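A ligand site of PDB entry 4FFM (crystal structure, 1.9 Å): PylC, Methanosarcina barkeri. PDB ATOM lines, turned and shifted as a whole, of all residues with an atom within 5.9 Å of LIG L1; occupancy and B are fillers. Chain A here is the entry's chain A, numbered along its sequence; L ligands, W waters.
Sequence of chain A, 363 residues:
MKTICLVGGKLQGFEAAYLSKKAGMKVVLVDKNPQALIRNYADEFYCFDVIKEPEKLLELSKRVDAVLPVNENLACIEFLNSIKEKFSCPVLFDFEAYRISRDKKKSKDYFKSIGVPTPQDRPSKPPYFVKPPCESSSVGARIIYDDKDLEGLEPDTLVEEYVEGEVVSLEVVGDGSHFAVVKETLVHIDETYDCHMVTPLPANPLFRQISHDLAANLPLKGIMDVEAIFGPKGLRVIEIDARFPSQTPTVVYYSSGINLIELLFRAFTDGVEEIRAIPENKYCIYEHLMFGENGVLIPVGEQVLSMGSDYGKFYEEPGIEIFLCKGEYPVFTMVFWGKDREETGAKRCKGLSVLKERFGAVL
O13 of LIG L1 is in hydrogen-bond range of OD1 of Asp 31 (2.7 Å).
The backbone NH of Glu 72 is in hydrogen-bond range of an oxygen (O7) of LIG L1 (2.8 Å).
N3 of LIG L1 is in hydrogen-bond range of OD1 of Asp 49 (2.8 Å).
The side-chain amino group (NZ) of Lys 10 lies within salt-bridge range of an oxygen (O4) of LIG L1 (2.9 Å).
ND2 of Asn 73 lies within hydrogen-bond range of N2 of LIG L1, at 3.0 Å.
N of Val 50 is in hydrogen-bond range of N4 of LIG L1.
The backbone NH (N) of Lys 32 sits at hydrogen-bond distance from a nitrogen (N5) of LIG L1 (3.2 Å).
The side-chain sulfur (SG) of Cys 76 sits close to a nitrogen (N3) of LIG L1, at 3.7 Å.
OE1 of Glu 72 is in salt-bridge range of N4 of LG2 L2, 2.8 Å away.
The backbone NH of Gln 12 is in hydrogen-bond range of an oxygen (O2) of LG2 L2.
The side-chain amide oxygen of Gln 12 sits at hydrogen-bond distance from a nitrogen (N4) of LG2 L2, at 2.9 Å.
O7 of LIG L1 sits at hydrogen-bond distance from N4 of LG2 L2 (2.7 Å).
The side-chain carboxylate (OD2) of Asp 31 is in hydrogen-bond range of the backbone NH (N) of Gly 9, at 2.8 Å.
The backbone NH of Asn 33 sits at hydrogen-bond distance from the side-chain carboxylate of Asp 31.
The backbone NH (N) of Asn 73 lies within hydrogen-bond range of the side-chain amide oxygen (OD1) of Asn 71 (3.0 Å).
The backbone carbonyl oxygen of Phe 48 sits at hydrogen-bond distance from the backbone NH of Lys 32, 3.4 Å away.
SG of Cys 76 lies within hydrogen-bond range of ND2 of Asn 71, at 3.5 Å.
The backbone NH of Asn 71 sits close to the side-chain amide oxygen of Gln 12, at 3.4 Å.
The side-chain amide nitrogen (ND2) of Asn 71 lies within hydrogen-bond range of the backbone carbonyl oxygen (O) of Val 7, 3.1 Å away.
The backbone carbonyl oxygen of Gly 9 is in hydrogen-bond range of the backbone NH of Leu 37 (3.4 Å).
Residues that only touch LIG L1: Gly 8 (3.4 Å), Asn 71 (3.4 Å), Phe 48 (3.5 Å), Ile 51 (3.6 Å) and Gly 9 (3.97 Å).
The nearest printed residue that does not touch LIG L1 is Asn 33 (4.01 Å).
Water W3 lies within hydrogen-bond range of O12 of LIG L1 (2.8 Å) and ND2 of Asn 33 (2.9 Å).
Water W4 lies within hydrogen-bond range of O3 of LG2 L2 (2.7 Å) and O4 of LIG L1 (2.8 Å).
Water W1 lies within hydrogen-bond range of O8 of LIG L1 (2.9 Å) and NZ of Lys 32 (3.2 Å).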
ATOM      1  N   VAL A   7      28.583 -20.111   0.919  1.00  0.00           N
ATOM      2  CA  VAL A   7      27.295 -19.741   1.527  1.00  0.00           C
ATOM      3  C   VAL A   7      27.544 -18.659   2.596  1.00  0.00           C
ATOM      4  O   VAL A   7      27.920 -18.970   3.727  1.00  0.00           O
ATOM      5  CB  VAL A   7      26.511 -20.972   2.098  1.00  0.00           C
ATOM      6  CG1 VAL A   7      25.188 -20.549   2.722  1.00  0.00           C
ATOM      7  CG2 VAL A   7      26.259 -22.020   1.018  1.00  0.00           C
ATOM      8  N   GLY A   8      27.365 -17.399   2.203  1.00  0.00           N
ATOM      9  CA  GLY A   8      27.667 -16.245   3.062  1.00  0.00           C
ATOM     10  C   GLY A   8      28.618 -15.286   2.394  1.00  0.00           C
ATOM     11  O   GLY A   8      29.729 -15.674   2.017  1.00  0.00           O
ATOM     12  N   GLY A   9      28.197 -14.034   2.235  1.00  0.00           N
ATOM     13  CA  GLY A   9      28.999 -13.025   1.529  1.00  0.00           C
ATOM     14  C   GLY A   9      29.330 -11.765   2.322  1.00  0.00           C
ATOM     15  O   GLY A   9      29.271 -10.659   1.797  1.00  0.00           O
ATOM     16  N   LYS A  10      29.663 -11.951   3.595  1.00  0.00           N
ATOM     17  CA  LYS A  10      30.180 -10.866   4.416  1.00  0.00           C
ATOM     18  C   LYS A  10      31.698 -11.033   4.665  1.00  0.00           C
ATOM     19  O   LYS A  10      32.450 -11.216   3.713  1.00  0.00           O
ATOM     20  CB  LYS A  10      29.364 -10.733   5.714  1.00  0.00           C
ATOM     21  CG  LYS A  10      28.337  -9.600   5.735  1.00  0.00           C
ATOM     22  CD  LYS A  10      27.595  -9.553   7.059  1.00  0.00           C
ATOM     23  CE  LYS A  10      27.419  -8.127   7.534  1.00  0.00           C
ATOM     24  NZ  LYS A  10      26.460  -8.002   8.665  1.00  0.00           N
ATOM     25  N   GLN A  12      33.723 -13.381   6.412  1.00  0.00           N
ATOM     26  CA  GLN A  12      34.285 -14.708   6.152  1.00  0.00           C
ATOM     27  C   GLN A  12      34.223 -14.979   4.648  1.00  0.00           C
ATOM     28  O   GLN A  12      35.156 -15.534   4.083  1.00  0.00           O
ATOM     29  CB  GLN A  12      33.494 -15.810   6.845  1.00  0.00           C
ATOM     30  CG  GLN A  12      33.466 -15.843   8.358  1.00  0.00           C
ATOM     31  CD  GLN A  12      32.548 -16.956   8.831  1.00  0.00           C
ATOM     32  OE1 GLN A  12      31.429 -16.708   9.260  1.00  0.00           O
ATOM     33  NE2 GLN A  12      33.005 -18.200   8.698  1.00  0.00           N
ATOM     34  N   VAL A  30      26.376 -17.624  -2.733  1.00  0.00           N
ATOM     35  CA  VAL A  30      24.982 -17.700  -2.332  1.00  0.00           C
ATOM     36  C   VAL A  30      24.798 -16.848  -1.055  1.00  0.00           C
ATOM     37  O   VAL A  30      25.528 -17.037  -0.074  1.00  0.00           O
ATOM     38  CB  VAL A  30      24.506 -19.163  -2.100  1.00  0.00           C
ATOM     39  CG1 VAL A  30      23.080 -19.197  -1.534  1.00  0.00           C
ATOM     40  CG2 VAL A  30      24.569 -19.978  -3.384  1.00  0.00           C
ATOM     41  N   ASP A  31      23.846 -15.910  -1.089  1.00  0.00           N
ATOM     42  CA  ASP A  31      23.500 -15.106   0.078  1.00  0.00           C
ATOM     43  C   ASP A  31      22.030 -14.640  -0.028  1.00  0.00           C
ATOM     44  O   ASP A  31      21.579 -14.272  -1.119  1.00  0.00           O
ATOM     45  CB  ASP A  31      24.448 -13.900   0.242  1.00  0.00           C
ATOM     46  CG  ASP A  31      24.460 -13.323   1.659  1.00  0.00           C
ATOM     47  OD1 ASP A  31      23.395 -12.893   2.143  1.00  0.00           O
ATOM     48  OD2 ASP A  31      25.526 -13.292   2.295  1.00  0.00           O
ATOM     49  N   LYS A  32      21.323 -14.673   1.112  1.00  0.00           N
ATOM     50  CA  LYS A  32      19.909 -14.272   1.233  1.00  0.00           C
ATOM     51  C   LYS A  32      19.703 -12.739   1.124  1.00  0.00           C
ATOM     52  O   LYS A  32      18.597 -12.272   0.804  1.00  0.00           O
ATOM     53  CB  LYS A  32      19.324 -14.804   2.566  1.00  0.00           C
ATOM     54  CG  LYS A  32      19.925 -14.165   3.832  1.00  0.00           C
ATOM     55  CD  LYS A  32      19.290 -14.659   5.127  1.00  0.00           C
ATOM     56  CE  LYS A  32      20.031 -14.132   6.352  1.00  0.00           C
ATOM     57  NZ  LYS A  32      19.577 -14.763   7.627  1.00  0.00           N
ATOM     58  N   ASN A  33      20.761 -11.971   1.399  1.00  0.00           N
ATOM     59  CA  ASN A  33      20.763 -10.494   1.302  1.00  0.00           C
ATOM     60  C   ASN A  33      21.054 -10.026  -0.142  1.00  0.00           C
ATOM     61  O   ASN A  33      22.164 -10.278  -0.654  1.00  0.00           O
ATOM     62  CB  ASN A  33      21.751  -9.882   2.334  1.00  0.00           C
ATOM     63  CG  ASN A  33      21.776  -8.346   2.343  1.00  0.00           C
ATOM     64  OD1 ASN A  33      21.163  -7.681   1.504  1.00  0.00           O
ATOM     65  ND2 ASN A  33      22.492  -7.772   3.315  1.00  0.00           N
ATOM     66  N   ALA A  36      24.219  -8.174  -0.416  1.00  0.00           N
ATOM     67  CA  ALA A  36      25.290  -8.867   0.314  1.00  0.00           C
ATOM     68  C   ALA A  36      26.601  -8.154   0.053  1.00  0.00           C
ATOM     69  O   ALA A  36      26.901  -7.779  -1.087  1.00  0.00           O
ATOM     70  CB  ALA A  36      25.384 -10.345  -0.056  1.00  0.00           C
ATOM     71  N   LEU A  37      27.385  -7.940   1.120  1.00  0.00           N
ATOM     72  CA  LEU A  37      28.639  -7.176   1.069  1.00  0.00           C
ATOM     73  C   LEU A  37      29.556  -7.461  -0.138  1.00  0.00           C
ATOM     74  O   LEU A  37      30.002  -6.512  -0.773  1.00  0.00           O
ATOM     75  CB  LEU A  37      29.400  -7.305   2.394  1.00  0.00           C
ATOM     76  CG  LEU A  37      30.653  -6.477   2.648  1.00  0.00           C
ATOM     77  CD1 LEU A  37      30.332  -4.983   2.678  1.00  0.00           C
ATOM     78  CD2 LEU A  37      31.264  -6.943   3.960  1.00  0.00           C
ATOM     79  N   PHE A  48      19.335 -16.135  -2.621  1.00  0.00           N
ATOM     80  CA  PHE A  48      18.290 -16.942  -1.991  1.00  0.00           C
ATOM     81  C   PHE A  48      18.715 -17.380  -0.594  1.00  0.00           C
ATOM     82  O   PHE A  48      19.917 -17.390  -0.270  1.00  0.00           O
ATOM     83  CB  PHE A  48      17.876 -18.139  -2.871  1.00  0.00           C
ATOM     84  CG  PHE A  48      18.931 -19.212  -3.035  1.00  0.00           C
ATOM     85  CD1 PHE A  48      19.868 -19.150  -4.075  1.00  0.00           C
ATOM     86  CD2 PHE A  48      18.949 -20.333  -2.197  1.00  0.00           C
ATOM     87  CE1 PHE A  48      20.832 -20.144  -4.234  1.00  0.00           C
ATOM     88  CE2 PHE A  48      19.902 -21.335  -2.351  1.00  0.00           C
ATOM     89  CZ  PHE A  48      20.836 -21.242  -3.363  1.00  0.00           C
ATOM     90  N   ASP A  49      17.723 -17.752   0.215  1.00  0.00           N
ATOM     91  CA  ASP A  49      17.955 -18.302   1.549  1.00  0.00           C
ATOM     92  C   ASP A  49      18.004 -19.832   1.421  1.00  0.00           C
ATOM     93  O   ASP A  49      17.035 -20.432   0.968  1.00  0.00           O
ATOM     94  CB  ASP A  49      16.839 -17.848   2.510  1.00  0.00           C
ATOM     95  CG  ASP A  49      17.122 -18.195   3.971  1.00  0.00           C
ATOM     96  OD1 ASP A  49      17.582 -19.313   4.236  1.00  0.00           O
ATOM     97  OD2 ASP A  49      16.877 -17.348   4.855  1.00  0.00           O
ATOM     98  N   VAL A  50      19.131 -20.433   1.799  1.00  0.00           N
ATOM     99  CA  VAL A  50      19.360 -21.875   1.606  1.00  0.00           C
ATOM    100  C   VAL A  50      18.381 -22.735   2.421  1.00  0.00           C
ATOM    101  O   VAL A  50      18.068 -23.865   2.044  1.00  0.00           O
ATOM    102  CB  VAL A  50      20.833 -22.319   1.838  1.00  0.00           C
ATOM    103  CG1 VAL A  50      21.809 -21.499   0.988  1.00  0.00           C
ATOM    104  CG2 VAL A  50      21.209 -22.258   3.313  1.00  0.00           C
ATOM    105  N   ILE A  51      17.896 -22.169   3.542  1.00  0.00           N
ATOM    106  CA  ILE A  51      16.905 -22.831   4.407  1.00  0.00           C
ATOM    107  C   ILE A  51      15.520 -22.869   3.746  1.00  0.00           C
ATOM    108  O   ILE A  51      14.810 -23.868   3.836  1.00  0.00           O
ATOM    109  CB  ILE A  51      16.791 -22.197   5.821  1.00  0.00           C
ATOM    110  CG1 ILE A  51      18.156 -22.070   6.529  1.00  0.00           C
ATOM    111  CG2 ILE A  51      15.812 -23.009   6.677  1.00  0.00           C
ATOM    112  CD1 ILE A  51      18.132 -21.200   7.785  1.00  0.00           C
ATOM    113  N   VAL A  70      30.278 -20.115   4.952  1.00  0.00           N
ATOM    114  CA  VAL A  70      31.039 -19.003   5.517  1.00  0.00           C
ATOM    115  C   VAL A  70      30.058 -18.006   6.165  1.00  0.00           C
ATOM    116  O   VAL A  70      29.901 -16.873   5.706  1.00  0.00           O
ATOM    117  CB  VAL A  70      32.008 -18.355   4.507  1.00  0.00           C
ATOM    118  CG1 VAL A  70      33.374 -19.028   4.532  1.00  0.00           C
ATOM    119  CG2 VAL A  70      31.440 -18.333   3.097  1.00  0.00           C
ATOM    120  N   ASN A  71      29.377 -18.495   7.196  1.00  0.00           N
ATOM    121  CA  ASN A  71      28.479 -17.706   8.043  1.00  0.00           C
ATOM    122  C   ASN A  71      28.363 -18.393   9.397  1.00  0.00           C
ATOM    123  O   ASN A  71      28.709 -19.573   9.545  1.00  0.00           O
ATOM    124  CB  ASN A  71      27.087 -17.477   7.399  1.00  0.00           C
ATOM    125  CG  ASN A  71      26.203 -18.713   7.375  1.00  0.00           C
ATOM    126  OD1 ASN A  71      25.601 -19.076   8.375  1.00  0.00           O
ATOM    127  ND2 ASN A  71      26.115 -19.367   6.213  1.00  0.00           N
ATOM    128  N   GLU A  72      27.880 -17.641  10.373  1.00  0.00           N
ATOM    129  CA  GLU A  72      27.718 -18.111  11.736  1.00  0.00           C
ATOM    130  C   GLU A  72      26.248 -17.926  12.142  1.00  0.00           C
ATOM    131  O   GLU A  72      25.934 -17.636  13.308  1.00  0.00           O
ATOM    132  CB  GLU A  72      28.658 -17.351  12.679  1.00  0.00           C
ATOM    133  CG  GLU A  72      30.135 -17.467  12.307  1.00  0.00           C
ATOM    134  CD  GLU A  72      31.028 -16.543  13.107  1.00  0.00           C
ATOM    135  OE1 GLU A  72      30.948 -15.309  12.914  1.00  0.00           O
ATOM    136  OE2 GLU A  72      31.831 -17.057  13.910  1.00  0.00           O
ATOM    137  N   ASN A  73      25.354 -18.083  11.165  1.00  0.00           N
ATOM    138  CA  ASN A  73      23.908 -18.180  11.464  1.00  0.00           C
ATOM    139  C   ASN A  73      23.610 -19.620  11.879  1.00  0.00           C
ATOM    140  O   ASN A  73      23.643 -20.526  11.041  1.00  0.00           O
ATOM    141  CB  ASN A  73      23.084 -17.725  10.239  1.00  0.00           C
ATOM    142  CG  ASN A  73      21.591 -18.024  10.360  1.00  0.00           C
ATOM    143  OD1 ASN A  73      21.087 -18.297  11.435  1.00  0.00           O
ATOM    144  ND2 ASN A  73      20.878 -17.950   9.244  1.00  0.00           N
ATOM    145  N   CYS A  76      21.159 -21.609   9.839  1.00  0.00           N
ATOM    146  CA  CYS A  76      21.744 -22.025   8.553  1.00  0.00           C
ATOM    147  C   CYS A  76      22.685 -23.232   8.711  1.00  0.00           C
ATOM    148  O   CYS A  76      22.510 -24.221   8.033  1.00  0.00           O
ATOM    149  CB  CYS A  76      22.447 -20.869   7.831  1.00  0.00           C
ATOM    150  SG  CYS A  76      23.186 -21.303   6.228  1.00  0.00           S
ATOM    151  N   SER A 306      31.914  -4.535   8.485  1.00  0.00           N
ATOM    152  CA  SER A 306      30.744  -5.363   8.240  1.00  0.00           C
ATOM    153  C   SER A 306      29.452  -4.544   8.110  1.00  0.00           C
ATOM    154  O   SER A 306      28.396  -5.113   7.873  1.00  0.00           O
ATOM    155  CB  SER A 306      30.565  -6.362   9.361  1.00  0.00           C
ATOM    156  OG  SER A 306      29.906  -5.715  10.441  1.00  0.00           O
HETATM  157  P1  LIG L   1      23.274 -10.569   9.659  1.00  0.00           P
HETATM  158  O1  LIG L   1      23.180  -9.088   9.372  1.00  0.00           O
HETATM  159  O2  LIG L   1      22.943 -10.923  11.091  1.00  0.00           O
HETATM  160  O3  LIG L   1      22.557 -11.417   8.624  1.00  0.00           O
HETATM  161  P2  LIG L   1      25.959 -11.270  10.558  1.00  0.00           P
HETATM  162  O4  LIG L   1      26.938 -10.122  10.609  1.00  0.00           O
HETATM  163  O5  LIG L   1      25.335 -11.800  11.836  1.00  0.00           O
HETATM  164  O6  LIG L   1      24.841 -10.949   9.426  1.00  0.00           O
HETATM  165  P3  LIG L   1      26.261 -14.014   9.668  1.00  0.00           P
HETATM  166  O7  LIG L   1      27.484 -14.905   9.835  1.00  0.00           O
HETATM  167  O8  LIG L   1      24.952 -14.379  10.319  1.00  0.00           O
HETATM  168  O9  LIG L   1      26.775 -12.504   9.916  1.00  0.00           O
HETATM  169  O10 LIG L   1      25.981 -14.048   8.094  1.00  0.00           O
HETATM  170  C1  LIG L   1      26.986 -13.698   7.136  1.00  0.00           C
HETATM  171  C2  LIG L   1      26.374 -13.702   5.751  1.00  0.00           C
HETATM  172  O11 LIG L   1      25.783 -14.989   5.541  1.00  0.00           O
HETATM  173  C3  LIG L   1      25.269 -12.660   5.659  1.00  0.00           C
HETATM  174  O12 LIG L   1      25.522 -11.838   4.513  1.00  0.00           O
HETATM  175  C4  LIG L   1      24.000 -13.476   5.533  1.00  0.00           C
HETATM  176  O13 LIG L   1      22.964 -12.839   4.758  1.00  0.00           O
HETATM  177  C5  LIG L   1      24.473 -14.841   5.007  1.00  0.00           C
HETATM  178  N1  LIG L   1      23.507 -15.898   5.419  1.00  0.00           N
HETATM  179  C6  LIG L   1      23.164 -16.229   6.684  1.00  0.00           C
HETATM  180  N2  LIG L   1      22.216 -17.198   6.696  1.00  0.00           N
HETATM  181  C7  LIG L   1      21.931 -17.496   5.410  1.00  0.00           C
HETATM  182  C8  LIG L   1      21.016 -18.441   4.708  1.00  0.00           C
HETATM  183  N3  LIG L   1      20.179 -19.262   5.399  1.00  0.00           N
HETATM  184  N4  LIG L   1      21.056 -18.424   3.355  1.00  0.00           N
HETATM  185  C9  LIG L   1      21.849 -17.613   2.637  1.00  0.00           C
HETATM  186  N5  LIG L   1      22.696 -16.731   3.213  1.00  0.00           N
HETATM  187  C10 LIG L   1      22.782 -16.640   4.566  1.00  0.00           C
HETATM  188  O1  LG2 L   2      37.804 -14.421  11.951  1.00  0.00           O
HETATM  189  C1  LG2 L   2      37.462 -13.446  12.592  1.00  0.00           C
HETATM  190  C2  LG2 L   2      38.525 -12.672  13.348  1.00  0.00           C
HETATM  191  C3  LG2 L   2      39.369 -13.557  14.312  1.00  0.00           C
HETATM  192  C4  LG2 L   2      40.368 -14.396  13.446  1.00  0.00           C
HETATM  193  C5  LG2 L   2      41.604 -15.015  14.136  1.00  0.00           C
HETATM  194  N1  LG2 L   2      42.015 -16.155  13.283  1.00  0.00           N
HETATM  195  N2  LG2 L   2      39.438 -12.173  12.309  1.00  0.00           N
HETATM  196  N3  LG2 L   2      36.192 -12.967  12.556  1.00  0.00           N
HETATM  197  C6  LG2 L   2      35.172 -13.503  11.665  1.00  0.00           C
HETATM  198  C7  LG2 L   2      33.881 -12.662  11.858  1.00  0.00           C
HETATM  199  C8  LG2 L   2      32.841 -12.967  10.753  1.00  0.00           C
HETATM  200  C9  LG2 L   2      31.442 -12.425  11.141  1.00  0.00           C
HETATM  201  C10 LG2 L   2      30.327 -12.948  10.199  1.00  0.00           C
HETATM  202  N4  LG2 L   2      30.126 -14.402  10.348  1.00  0.00           N
HETATM  203  C11 LG2 L   2      30.648 -12.596   8.764  1.00  0.00           C
HETATM  204  O2  LG2 L   2      30.967 -13.507   7.965  1.00  0.00           O
HETATM  205  O3  LG2 L   2      30.603 -11.387   8.421  1.00  0.00           O
HETATM  206  O   HOH W   1      22.337 -14.255   9.132  1.00  0.00           O
HETATM  207  O   HOH W   2      18.441 -17.194   7.321  1.00  0.00           O
HETATM  208  O   HOH W   3      24.181  -9.442   5.053  1.00  0.00           O
HETATM  209  O   HOH W   4      29.701  -9.559  10.208  1.00  0.00           O
